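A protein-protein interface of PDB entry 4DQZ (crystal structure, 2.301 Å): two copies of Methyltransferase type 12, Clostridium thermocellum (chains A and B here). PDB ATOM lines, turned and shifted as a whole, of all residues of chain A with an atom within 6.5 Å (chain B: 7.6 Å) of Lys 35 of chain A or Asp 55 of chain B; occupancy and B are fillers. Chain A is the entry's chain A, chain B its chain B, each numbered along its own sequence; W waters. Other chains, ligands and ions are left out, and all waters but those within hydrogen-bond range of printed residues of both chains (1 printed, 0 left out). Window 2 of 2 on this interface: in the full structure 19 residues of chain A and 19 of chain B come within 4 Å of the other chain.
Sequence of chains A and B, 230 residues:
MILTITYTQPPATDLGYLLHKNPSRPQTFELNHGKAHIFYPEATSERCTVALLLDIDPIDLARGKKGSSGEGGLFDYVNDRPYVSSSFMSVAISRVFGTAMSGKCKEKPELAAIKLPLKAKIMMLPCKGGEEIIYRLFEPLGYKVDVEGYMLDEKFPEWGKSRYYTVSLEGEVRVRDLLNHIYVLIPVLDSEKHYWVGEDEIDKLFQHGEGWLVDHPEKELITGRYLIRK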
ATOM      1  N   THR A  28      19.139  -0.608 -24.657  1.00  0.00           N
ATOM      2  CA  THR A  28      20.585  -0.708 -24.601  1.00  0.00           C
ATOM      3  C   THR A  28      21.029  -1.152 -23.217  1.00  0.00           C
ATOM      4  O   THR A  28      20.439  -0.767 -22.215  1.00  0.00           O
ATOM      5  CB  THR A  28      21.232   0.611 -24.957  1.00  0.00           C
ATOM      6  OG1 THR A  28      20.725   1.032 -26.222  1.00  0.00           O
ATOM      7  CG2 THR A  28      22.728   0.452 -25.064  1.00  0.00           C
ATOM      8  N   PHE A  29      22.055  -1.997 -23.185  1.00  0.00           N
ATOM      9  CA  PHE A  29      22.595  -2.524 -21.954  1.00  0.00           C
ATOM     10  C   PHE A  29      24.060  -2.170 -21.896  1.00  0.00           C
ATOM     11  O   PHE A  29      24.795  -2.397 -22.859  1.00  0.00           O
ATOM     12  CB  PHE A  29      22.411  -4.039 -21.897  1.00  0.00           C
ATOM     13  CG  PHE A  29      20.979  -4.459 -21.844  1.00  0.00           C
ATOM     14  CD1 PHE A  29      20.351  -4.665 -20.630  1.00  0.00           C
ATOM     15  CD2 PHE A  29      20.251  -4.621 -23.010  1.00  0.00           C
ATOM     16  CE1 PHE A  29      19.027  -5.040 -20.577  1.00  0.00           C
ATOM     17  CE2 PHE A  29      18.931  -4.992 -22.967  1.00  0.00           C
ATOM     18  CZ  PHE A  29      18.316  -5.207 -21.746  1.00  0.00           C
ATOM     19  N   GLU A  30      24.468  -1.584 -20.773  1.00  0.00           N
ATOM     20  CA  GLU A  30      25.862  -1.230 -20.548  1.00  0.00           C
ATOM     21  C   GLU A  30      26.543  -2.446 -19.970  1.00  0.00           C
ATOM     22  O   GLU A  30      26.027  -3.072 -19.047  1.00  0.00           O
ATOM     23  CB  GLU A  30      25.962  -0.066 -19.568  1.00  0.00           C
ATOM     24  CG  GLU A  30      25.210   1.177 -20.006  1.00  0.00           C
ATOM     25  CD  GLU A  30      25.917   1.911 -21.125  1.00  0.00           C
ATOM     26  OE1 GLU A  30      27.135   1.685 -21.297  1.00  0.00           O
ATOM     27  OE2 GLU A  30      25.259   2.709 -21.831  1.00  0.00           O
ATOM     28  N   LEU A  31      27.693  -2.795 -20.520  1.00  0.00           N
ATOM     29  CA  LEU A  31      28.376  -3.994 -20.074  1.00  0.00           C
ATOM     30  C   LEU A  31      29.764  -3.683 -19.550  1.00  0.00           C
ATOM     31  O   LEU A  31      30.213  -2.537 -19.536  1.00  0.00           O
ATOM     32  CB  LEU A  31      28.464  -4.993 -21.230  1.00  0.00           C
ATOM     33  CG  LEU A  31      27.106  -5.394 -21.807  1.00  0.00           C
ATOM     34  CD1 LEU A  31      27.262  -5.917 -23.213  1.00  0.00           C
ATOM     35  CD2 LEU A  31      26.440  -6.435 -20.926  1.00  0.00           C
ATOM     36  N   ASN A  32      30.447  -4.718 -19.103  1.00  0.00           N
ATOM     37  CA  ASN A  32      31.862  -4.579 -18.934  1.00  0.00           C
ATOM     38  C   ASN A  32      32.434  -4.193 -20.292  1.00  0.00           C
ATOM     39  O   ASN A  32      32.467  -5.016 -21.212  1.00  0.00           O
ATOM     40  CB  ASN A  32      32.465  -5.898 -18.457  1.00  0.00           C
ATOM     41  CG  ASN A  32      32.227  -6.151 -16.988  1.00  0.00           C
ATOM     42  OD1 ASN A  32      32.439  -5.280 -16.146  1.00  0.00           O
ATOM     43  ND2 ASN A  32      31.789  -7.353 -16.671  1.00  0.00           N
ATOM     44  N   HIS A  33      32.994  -2.988 -20.383  1.00  0.00           N
ATOM     45  CA  HIS A  33      33.720  -2.518 -21.584  1.00  0.00           C
ATOM     46  C   HIS A  33      32.978  -2.654 -22.924  1.00  0.00           C
ATOM     47  O   HIS A  33      33.523  -3.171 -23.895  1.00  0.00           O
ATOM     48  CB  HIS A  33      35.234  -2.944 -21.704  1.00  0.00           C
ATOM     49  CG  HIS A  33      35.647  -4.224 -20.998  1.00  0.00           C
ATOM     50  ND1 HIS A  33      34.789  -5.038 -20.296  1.00  0.00           N
ATOM     51  CD2 HIS A  33      36.851  -4.840 -20.937  1.00  0.00           C
ATOM     52  CE1 HIS A  33      35.444  -6.064 -19.789  1.00  0.00           C
ATOM     53  NE2 HIS A  33      36.697  -5.980 -20.180  1.00  0.00           N
ATOM     54  N   GLY A  34      31.741  -2.165 -22.971  1.00  0.00           N
ATOM     55  CA  GLY A  34      31.000  -2.110 -24.218  1.00  0.00           C
ATOM     56  C   GLY A  34      29.503  -1.985 -24.019  1.00  0.00           C
ATOM     57  O   GLY A  34      29.028  -1.976 -22.881  1.00  0.00           O
ATOM     58  N   LYS A  35      28.765  -1.887 -25.130  1.00  0.00           N
ATOM     59  CA  LYS A  35      27.298  -1.848 -25.103  1.00  0.00           C
ATOM     60  C   LYS A  35      26.695  -3.009 -25.881  1.00  0.00           C
ATOM     61  O   LYS A  35      27.290  -3.499 -26.842  1.00  0.00           O
ATOM     62  CB  LYS A  35      26.759  -0.548 -25.711  1.00  0.00           C
ATOM     63  CG  LYS A  35      27.433   0.727 -25.262  1.00  0.00           C
ATOM     64  CD  LYS A  35      26.536   1.916 -25.522  1.00  0.00           C
ATOM     65  CE  LYS A  35      27.226   3.225 -25.163  1.00  0.00           C
ATOM     66  NZ  LYS A  35      26.249   4.334 -24.995  1.00  0.00           N
ATOM     67  N   ALA A  36      25.506  -3.429 -25.455  1.00  0.00           N
ATOM     68  CA  ALA A  36      24.660  -4.327 -26.228  1.00  0.00           C
ATOM     69  C   ALA A  36      23.345  -3.625 -26.574  1.00  0.00           C
ATOM     70  O   ALA A  36      22.673  -3.091 -25.703  1.00  0.00           O
ATOM     71  CB  ALA A  36      24.386  -5.609 -25.461  1.00  0.00           C
ATOM     72  N   HIS A  37      22.992  -3.613 -27.855  1.00  0.00           N
ATOM     73  CA  HIS A  37      21.733  -3.030 -28.299  1.00  0.00           C
ATOM     74  C   HIS A  37      20.831  -4.186 -28.729  1.00  0.00           C
ATOM     75  O   HIS A  37      21.274  -5.117 -29.398  1.00  0.00           O
ATOM     76  CB  HIS A  37      21.983  -2.119 -29.505  1.00  0.00           C
ATOM     77  CG  HIS A  37      23.014  -1.065 -29.261  1.00  0.00           C
ATOM     78  ND1 HIS A  37      22.753   0.074 -28.527  1.00  0.00           N
ATOM     79  CD2 HIS A  37      24.304  -0.973 -29.658  1.00  0.00           C
ATOM     80  CE1 HIS A  37      23.843   0.819 -28.482  1.00  0.00           C
ATOM     81  NE2 HIS A  37      24.793   0.212 -29.167  1.00  0.00           N
ATOM     82  N   LEU A  53      23.109  -6.402 -31.003  1.00  0.00           N
ATOM     83  CA  LEU A  53      24.272  -5.862 -31.671  1.00  0.00           C
ATOM     84  C   LEU A  53      25.269  -5.529 -30.575  1.00  0.00           C
ATOM     85  O   LEU A  53      24.919  -4.871 -29.596  1.00  0.00           O
ATOM     86  CB  LEU A  53      23.851  -4.646 -32.498  1.00  0.00           C
ATOM     87  CG  LEU A  53      24.900  -3.872 -33.287  1.00  0.00           C
ATOM     88  CD1 LEU A  53      24.261  -3.315 -34.566  1.00  0.00           C
ATOM     89  CD2 LEU A  53      25.463  -2.758 -32.423  1.00  0.00           C
ATOM     90  N   LEU A  54      26.489  -6.034 -30.704  1.00  0.00           N
ATOM     91  CA  LEU A  54      27.520  -5.779 -29.683  1.00  0.00           C
ATOM     92  C   LEU A  54      28.468  -4.664 -30.076  1.00  0.00           C
ATOM     93  O   LEU A  54      29.034  -4.660 -31.162  1.00  0.00           O
ATOM     94  CB  LEU A  54      28.369  -7.009 -29.452  1.00  0.00           C
ATOM     95  CG  LEU A  54      27.657  -8.263 -29.022  1.00  0.00           C
ATOM     96  CD1 LEU A  54      28.712  -9.190 -28.470  1.00  0.00           C
ATOM     97  CD2 LEU A  54      26.594  -7.943 -28.003  1.00  0.00           C
ATOM     98  N   ASP A  55      28.660  -3.725 -29.175  1.00  0.00           N
ATOM     99  CA  ASP A  55      29.588  -2.641 -29.448  1.00  0.00           C
ATOM    100  C   ASP A  55      30.644  -2.674 -28.351  1.00  0.00           C
ATOM    101  O   ASP A  55      30.364  -2.307 -27.213  1.00  0.00           O
ATOM    102  CB  ASP A  55      28.815  -1.319 -29.466  1.00  0.00           C
ATOM    103  CG  ASP A  55      29.694  -0.117 -29.700  1.00  0.00           C
ATOM    104  OD1 ASP A  55      30.812  -0.270 -30.244  1.00  0.00           O
ATOM    105  OD2 ASP A  55      29.235   0.992 -29.347  1.00  0.00           O
ATOM    106  N   ILE A  56      31.844  -3.146 -28.688  1.00  0.00           N
ATOM    107  CA  ILE A  56      32.909  -3.313 -27.696  1.00  0.00           C
ATOM    108  C   ILE A  56      33.939  -2.181 -27.716  1.00  0.00           C
ATOM    109  O   ILE A  56      34.328  -1.717 -28.790  1.00  0.00           O
ATOM    110  CB  ILE A  56      33.623  -4.662 -27.860  1.00  0.00           C
ATOM    111  CG1 ILE A  56      32.592  -5.772 -28.067  1.00  0.00           C
ATOM    112  CG2 ILE A  56      34.489  -4.962 -26.642  1.00  0.00           C
ATOM    113  CD1 ILE A  56      33.184  -7.066 -28.569  1.00  0.00           C
ATOM    114  N   ASP A  57      34.358  -1.796 -26.501  1.00  0.00           N
ATOM    115  CA  ASP A  57      35.209  -0.644 -26.133  1.00  0.00           C
ATOM    116  C   ASP A  57      34.379   0.498 -25.551  1.00  0.00           C
ATOM    117  O   ASP A  57      33.849   0.385 -24.443  1.00  0.00           O
ATOM    118  CB  ASP A  57      36.142  -0.147 -27.249  1.00  0.00           C
ATOM    119  CG  ASP A  57      37.375  -1.013 -27.404  1.00  0.00           C
ATOM    120  OD1 ASP A  57      37.317  -2.205 -27.023  1.00  0.00           O
ATOM    121  OD2 ASP A  57      38.403  -0.503 -27.902  1.00  0.00           O
ATOM    122  N   PHE A  88      32.270 -12.141 -25.032  1.00  0.00           N
ATOM    123  CA  PHE A  88      31.454 -10.946 -24.798  1.00  0.00           C
ATOM    124  C   PHE A  88      30.006 -11.151 -25.266  1.00  0.00           C
ATOM    125  O   PHE A  88      29.071 -10.664 -24.632  1.00  0.00           O
ATOM    126  CB  PHE A  88      32.096  -9.736 -25.491  1.00  0.00           C
ATOM    127  CG  PHE A  88      31.507  -8.404 -25.091  1.00  0.00           C
ATOM    128  CD1 PHE A  88      31.865  -7.799 -23.897  1.00  0.00           C
ATOM    129  CD2 PHE A  88      30.618  -7.744 -25.928  1.00  0.00           C
ATOM    130  CE1 PHE A  88      31.329  -6.573 -23.539  1.00  0.00           C
ATOM    131  CE2 PHE A  88      30.083  -6.518 -25.576  1.00  0.00           C
ATOM    132  CZ  PHE A  88      30.441  -5.933 -24.383  1.00  0.00           C
ATOM    133  N   MET B   1      17.961   6.365 -32.043  1.00  0.00           N
ATOM    134  CA  MET B   1      16.813   5.876 -32.783  1.00  0.00           C
ATOM    135  C   MET B   1      17.285   4.944 -33.894  1.00  0.00           C
ATOM    136  O   MET B   1      18.469   4.835 -34.150  1.00  0.00           O
ATOM    137  CB  MET B   1      15.931   7.044 -33.319  1.00  0.00           C
ATOM    138  CG  MET B   1      16.435   7.805 -34.551  1.00  0.00           C
ATOM    139  SD  MET B   1      15.347   9.126 -35.273  1.00  0.00           S
ATOM    140  CE  MET B   1      15.270  10.206 -33.846  1.00  0.00           C
ATOM    141  N   PHE B  29      30.213   3.821 -37.930  1.00  0.00           N
ATOM    142  CA  PHE B  29      30.658   5.143 -38.301  1.00  0.00           C
ATOM    143  C   PHE B  29      30.690   5.997 -37.057  1.00  0.00           C
ATOM    144  O   PHE B  29      29.717   6.037 -36.300  1.00  0.00           O
ATOM    145  CB  PHE B  29      29.713   5.749 -39.334  1.00  0.00           C
ATOM    146  CG  PHE B  29      29.712   5.017 -40.636  1.00  0.00           C
ATOM    147  CD1 PHE B  29      30.556   5.402 -41.660  1.00  0.00           C
ATOM    148  CD2 PHE B  29      28.883   3.925 -40.827  1.00  0.00           C
ATOM    149  CE1 PHE B  29      30.564   4.721 -42.857  1.00  0.00           C
ATOM    150  CE2 PHE B  29      28.886   3.242 -42.016  1.00  0.00           C
ATOM    151  CZ  PHE B  29      29.727   3.642 -43.038  1.00  0.00           C
ATOM    152  N   LEU B  31      30.657   9.510 -35.286  1.00  0.00           N
ATOM    153  CA  LEU B  31      30.064  10.781 -35.657  1.00  0.00           C
ATOM    154  C   LEU B  31      30.417  11.872 -34.662  1.00  0.00           C
ATOM    155  O   LEU B  31      31.112  11.643 -33.671  1.00  0.00           O
ATOM    156  CB  LEU B  31      28.544  10.628 -35.750  1.00  0.00           C
ATOM    157  CG  LEU B  31      28.083   9.572 -36.754  1.00  0.00           C
ATOM    158  CD1 LEU B  31      26.690   9.101 -36.426  1.00  0.00           C
ATOM    159  CD2 LEU B  31      28.136  10.124 -38.169  1.00  0.00           C
ATOM    160  N   ASN B  32      29.943  13.071 -34.935  1.00  0.00           N
ATOM    161  CA  ASN B  32      29.925  14.056 -33.892  1.00  0.00           C
ATOM    162  C   ASN B  32      29.102  13.459 -32.752  1.00  0.00           C
ATOM    163  O   ASN B  32      27.885  13.308 -32.876  1.00  0.00           O
ATOM    164  CB  ASN B  32      29.281  15.348 -34.395  1.00  0.00           C
ATOM    165  CG  ASN B  32      30.203  16.161 -35.276  1.00  0.00           C
ATOM    166  OD1 ASN B  32      31.361  16.399 -34.934  1.00  0.00           O
ATOM    167  ND2 ASN B  32      29.689  16.597 -36.422  1.00  0.00           N
ATOM    168  N   HIS B  33      29.741  13.230 -31.607  1.00  0.00           N
ATOM    169  CA  HIS B  33      29.053  12.797 -30.371  1.00  0.00           C
ATOM    170  C   HIS B  33      28.120  11.579 -30.497  1.00  0.00           C
ATOM    171  O   HIS B  33      26.977  11.616 -30.051  1.00  0.00           O
ATOM    172  CB  HIS B  33      28.422  13.938 -29.480  1.00  0.00           C
ATOM    173  CG  HIS B  33      27.967  15.197 -30.195  1.00  0.00           C
ATOM    174  ND1 HIS B  33      28.151  15.435 -31.539  1.00  0.00           N
ATOM    175  CD2 HIS B  33      27.378  16.317 -29.714  1.00  0.00           C
ATOM    176  CE1 HIS B  33      27.654  16.610 -31.867  1.00  0.00           C
ATOM    177  NE2 HIS B  33      27.201  17.182 -30.770  1.00  0.00           N
ATOM    178  N   GLY B  34      28.628  10.497 -31.082  1.00  0.00           N
ATOM    179  CA  GLY B  34      27.892   9.245 -31.124  1.00  0.00           C
ATOM    180  C   GLY B  34      28.368   8.300 -32.211  1.00  0.00           C
ATOM    181  O   GLY B  34      29.280   8.636 -32.970  1.00  0.00           O
ATOM    182  N   LYS B  35      27.746   7.119 -32.281  1.00  0.00           N
ATOM    183  CA  LYS B  35      28.035   6.137 -33.332  1.00  0.00           C
ATOM    184  C   LYS B  35      26.795   5.824 -34.158  1.00  0.00           C
ATOM    185  O   LYS B  35      25.673   5.897 -33.657  1.00  0.00           O
ATOM    186  CB  LYS B  35      28.553   4.820 -32.741  1.00  0.00           C
ATOM    187  CG  LYS B  35      29.617   4.942 -31.676  1.00  0.00           C
ATOM    188  CD  LYS B  35      30.380   3.646 -31.536  1.00  0.00           C
ATOM    189  CE  LYS B  35      31.398   3.714 -30.408  1.00  0.00           C
ATOM    190  NZ  LYS B  35      32.425   2.645 -30.533  1.00  0.00           N
ATOM    191  N   ALA B  36      27.021   5.470 -35.422  1.00  0.00           N
ATOM    192  CA  ALA B  36      26.004   4.870 -36.273  1.00  0.00           C
ATOM    193  C   ALA B  36      26.444   3.462 -36.688  1.00  0.00           C
ATOM    194  O   ALA B  36      27.545   3.273 -37.187  1.00  0.00           O
ATOM    195  CB  ALA B  36      25.752   5.728 -37.503  1.00  0.00           C
ATOM    196  N   HIS B  37      25.583   2.474 -36.466  1.00  0.00           N
ATOM    197  CA  HIS B  37      25.869   1.106 -36.875  1.00  0.00           C
ATOM    198  C   HIS B  37      24.937   0.785 -38.040  1.00  0.00           C
ATOM    199  O   HIS B  37      23.755   1.118 -38.005  1.00  0.00           O
ATOM    200  CB  HIS B  37      25.562   0.150 -35.719  1.00  0.00           C
ATOM    201  CG  HIS B  37      26.269   0.495 -34.449  1.00  0.00           C
ATOM    202  ND1 HIS B  37      27.607   0.227 -34.247  1.00  0.00           N
ATOM    203  CD2 HIS B  37      25.824   1.079 -33.313  1.00  0.00           C
ATOM    204  CE1 HIS B  37      27.953   0.637 -33.042  1.00  0.00           C
ATOM    205  NE2 HIS B  37      26.889   1.148 -32.451  1.00  0.00           N
ATOM    206  N   LEU B  52      19.865   0.895 -39.544  1.00  0.00           N
ATOM    207  CA  LEU B  52      20.857   1.878 -39.163  1.00  0.00           C
ATOM    208  C   LEU B  52      20.515   2.305 -37.754  1.00  0.00           C
ATOM    209  O   LEU B  52      19.465   2.873 -37.487  1.00  0.00           O
ATOM    210  CB  LEU B  52      20.839   3.065 -40.107  1.00  0.00           C
ATOM    211  CG  LEU B  52      21.704   4.272 -39.722  1.00  0.00           C
ATOM    212  CD1 LEU B  52      23.190   3.952 -39.781  1.00  0.00           C
ATOM    213  CD2 LEU B  52      21.377   5.431 -40.630  1.00  0.00           C
ATOM    214  N   LEU B  53      21.415   2.005 -36.845  1.00  0.00           N
ATOM    215  CA  LEU B  53      21.102   2.146 -35.440  1.00  0.00           C
ATOM    216  C   LEU B  53      21.951   3.300 -34.930  1.00  0.00           C
ATOM    217  O   LEU B  53      23.158   3.337 -35.165  1.00  0.00           O
ATOM    218  CB  LEU B  53      21.387   0.822 -34.731  1.00  0.00           C
ATOM    219  CG  LEU B  53      21.158   0.705 -33.229  1.00  0.00           C
ATOM    220  CD1 LEU B  53      20.714  -0.721 -32.894  1.00  0.00           C
ATOM    221  CD2 LEU B  53      22.436   1.066 -32.494  1.00  0.00           C
ATOM    222  N   LEU B  54      21.315   4.274 -34.288  1.00  0.00           N
ATOM    223  CA  LEU B  54      22.051   5.440 -33.765  1.00  0.00           C
ATOM    224  C   LEU B  54      22.353   5.329 -32.287  1.00  0.00           C
ATOM    225  O   LEU B  54      21.474   5.075 -31.472  1.00  0.00           O
ATOM    226  CB  LEU B  54      21.260   6.715 -33.949  1.00  0.00           C
ATOM    227  CG  LEU B  54      20.849   7.066 -35.356  1.00  0.00           C
ATOM    228  CD1 LEU B  54      20.446   8.521 -35.343  1.00  0.00           C
ATOM    229  CD2 LEU B  54      21.976   6.797 -36.326  1.00  0.00           C
ATOM    230  N   ASP B  55      23.602   5.543 -31.935  1.00  0.00           N
ATOM    231  CA  ASP B  55      23.975   5.504 -30.533  1.00  0.00           C
ATOM    232  C   ASP B  55      24.575   6.863 -30.189  1.00  0.00           C
ATOM    233  O   ASP B  55      25.695   7.167 -30.598  1.00  0.00           O
ATOM    234  CB  ASP B  55      24.967   4.361 -30.314  1.00  0.00           C
ATOM    235  CG  ASP B  55      25.459   4.264 -28.895  1.00  0.00           C
ATOM    236  OD1 ASP B  55      24.775   4.772 -27.972  1.00  0.00           O
ATOM    237  OD2 ASP B  55      26.536   3.650 -28.715  1.00  0.00           O
ATOM    238  N   ILE B  56      23.813   7.689 -29.471  1.00  0.00           N
ATOM    239  CA  ILE B  56      24.237   9.058 -29.161  1.00  0.00           C
ATOM    240  C   ILE B  56      24.808   9.211 -27.750  1.00  0.00           C
ATOM    241  O   ILE B  56      24.277   8.629 -26.802  1.00  0.00           O
ATOM    242  CB  ILE B  56      23.092  10.061 -29.369  1.00  0.00           C
ATOM    243  CG1 ILE B  56      22.373   9.765 -30.685  1.00  0.00           C
ATOM    244  CG2 ILE B  56      23.622  11.488 -29.367  1.00  0.00           C
ATOM    245  CD1 ILE B  56      21.046  10.466 -30.823  1.00  0.00           C
ATOM    246  N   ASP B  57      25.873  10.020 -27.669  1.00  0.00           N
ATOM    247  CA  ASP B  57      26.768  10.268 -26.518  1.00  0.00           C
ATOM    248  C   ASP B  57      28.093   9.523 -26.668  1.00  0.00           C
ATOM    249  O   ASP B  57      28.913   9.867 -27.523  1.00  0.00           O
ATOM    250  CB  ASP B  57      26.134  10.012 -25.142  1.00  0.00           C
ATOM    251  CG  ASP B  57      25.234  11.148 -24.695  1.00  0.00           C
ATOM    252  OD1 ASP B  57      24.723  11.879 -25.572  1.00  0.00           O
ATOM    253  OD2 ASP B  57      25.041  11.312 -23.469  1.00  0.00           O
ATOM    254  N   PHE B  88      20.366  14.263 -35.751  1.00  0.00           N
ATOM    255  CA  PHE B  88      21.472  13.307 -35.731  1.00  0.00           C
ATOM    256  C   PHE B  88      21.235  12.161 -36.724  1.00  0.00           C
ATOM    257  O   PHE B  88      22.173  11.675 -37.354  1.00  0.00           O
ATOM    258  CB  PHE B  88      21.672  12.773 -34.306  1.00  0.00           C
ATOM    259  CG  PHE B  88      22.951  11.994 -34.107  1.00  0.00           C
ATOM    260  CD1 PHE B  88      24.161  12.648 -33.936  1.00  0.00           C
ATOM    261  CD2 PHE B  88      22.936  10.607 -34.059  1.00  0.00           C
ATOM    262  CE1 PHE B  88      25.330  11.930 -33.744  1.00  0.00           C
ATOM    263  CE2 PHE B  88      24.102   9.886 -33.864  1.00  0.00           C
ATOM    264  CZ  PHE B  88      25.296  10.549 -33.704  1.00  0.00           C
HETATM  265  O   HOH W   1      26.752   1.418 -29.993  1.00  0.00           O
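OD1 of Asp 55 of chain B is in salt-bridge range of NZ of Lys 35 of chain A (3.4 Å). NZ of Lys 35 of chain B is in salt-bridge range of OD1 of Asp 55 of chain A (3.3 Å).
ND1 of His 37 of chain A is in hydrogen-bond range of OG1 of Thr 28 of chain A. N of Lys 35 of chain B sits at hydrogen-bond distance from O of Asp 55 of chain B, 2.7 Å away. The backbone carbonyl oxygen of His 37 of chain A sits at hydrogen-bond distance from the backbone NH of Leu 53 of chain A (2.8 Å). The side-chain carboxylate (OE2) of Glu 30 of chain A is in salt-bridge range of the side-chain amino group (NZ) of Lys 35 of chain A (3.7 Å). The backbone carbonyl oxygen of His 37 of chain B lies within hydrogen-bond range of the backbone NH of Leu 53 of chain B. The backbone NH (N) of Lys 35 of chain A sits at hydrogen-bond distance from the backbone carbonyl oxygen (O) of Asp 55 of chain A (2.7 Å).
Lys 35 of chain A touches Asp 55 of chain B, and with the chains exchanged Asp 55 of chain A touches Lys 35 of chain B. His 37 of chain A touches Leu 53 of chain B, and with the chains exchanged Leu 53 of chain A touches His 37 of chain B. His 37 of chain A touches Asp 55 of chain B, and with the chains exchanged Asp 55 of chain A touches His 37 of chain B. Asp 55 of chain A touches its own counterpart, Asp 55 of chain B. Of the 7 pairs that touch across the chains among the printed residues, 7 have their exchanged pair printed and touching as well.
Of the 16 printed residues of chain A, 4 touch a printed residue of chain B. Hydrophobic or aromatic side chains of chain A that line the printed part of chain B: His 37 and Leu 53.
Water W1 lies within hydrogen-bond range of NE2 of His 37 of chain A (2.4 Å), NE2 of His 37 of chain B (2.5 Å), OD2 of Asp 55 of chain B (2.6 Å) and OD2 of Asp 55 of chain A (2.6 Å).
Glu 30 of chain A touches none of the printed residues of chain B. Of the printed residues of chain B, His 37 of chain A touches Leu 53 and Asp 55. Of the printed residues of chain B, Leu 53 of chain A touches His 37 (3.9 Å). Of the printed residues of chain B, Asp 55 of chain A touches Lys 35, His 37 and Asp 55. Of the printed residues of chain A, Leu 53 of chain B touches His 37 (3.9 Å). Of the printed residues of chain A, Asp 55 of chain B touches Lys 35 (3.4 Å), His 37 (3.8 Å) and Asp 55 (3.8 Å). Phe 88 of chain B touches none of the printed residues of chain A. The nearest residue of chain B that does not touch Lys 35 of chain A is Ile 56 of chain B (5.1 Å).
Among the printed residues, merely in contact across the chains: His 37 of chain A with Leu 53 of chain B (3.9 Å), His 37 of chain A with Asp 55 of chain B (3.8 Å), Leu 53 of chain A with His 37 of chain B (3.9 Å), Asp 55 of chain A with His 37 of chain B (3.8 Å) and Asp 55 of chain A with Asp 55 of chain B (3.8 Å).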
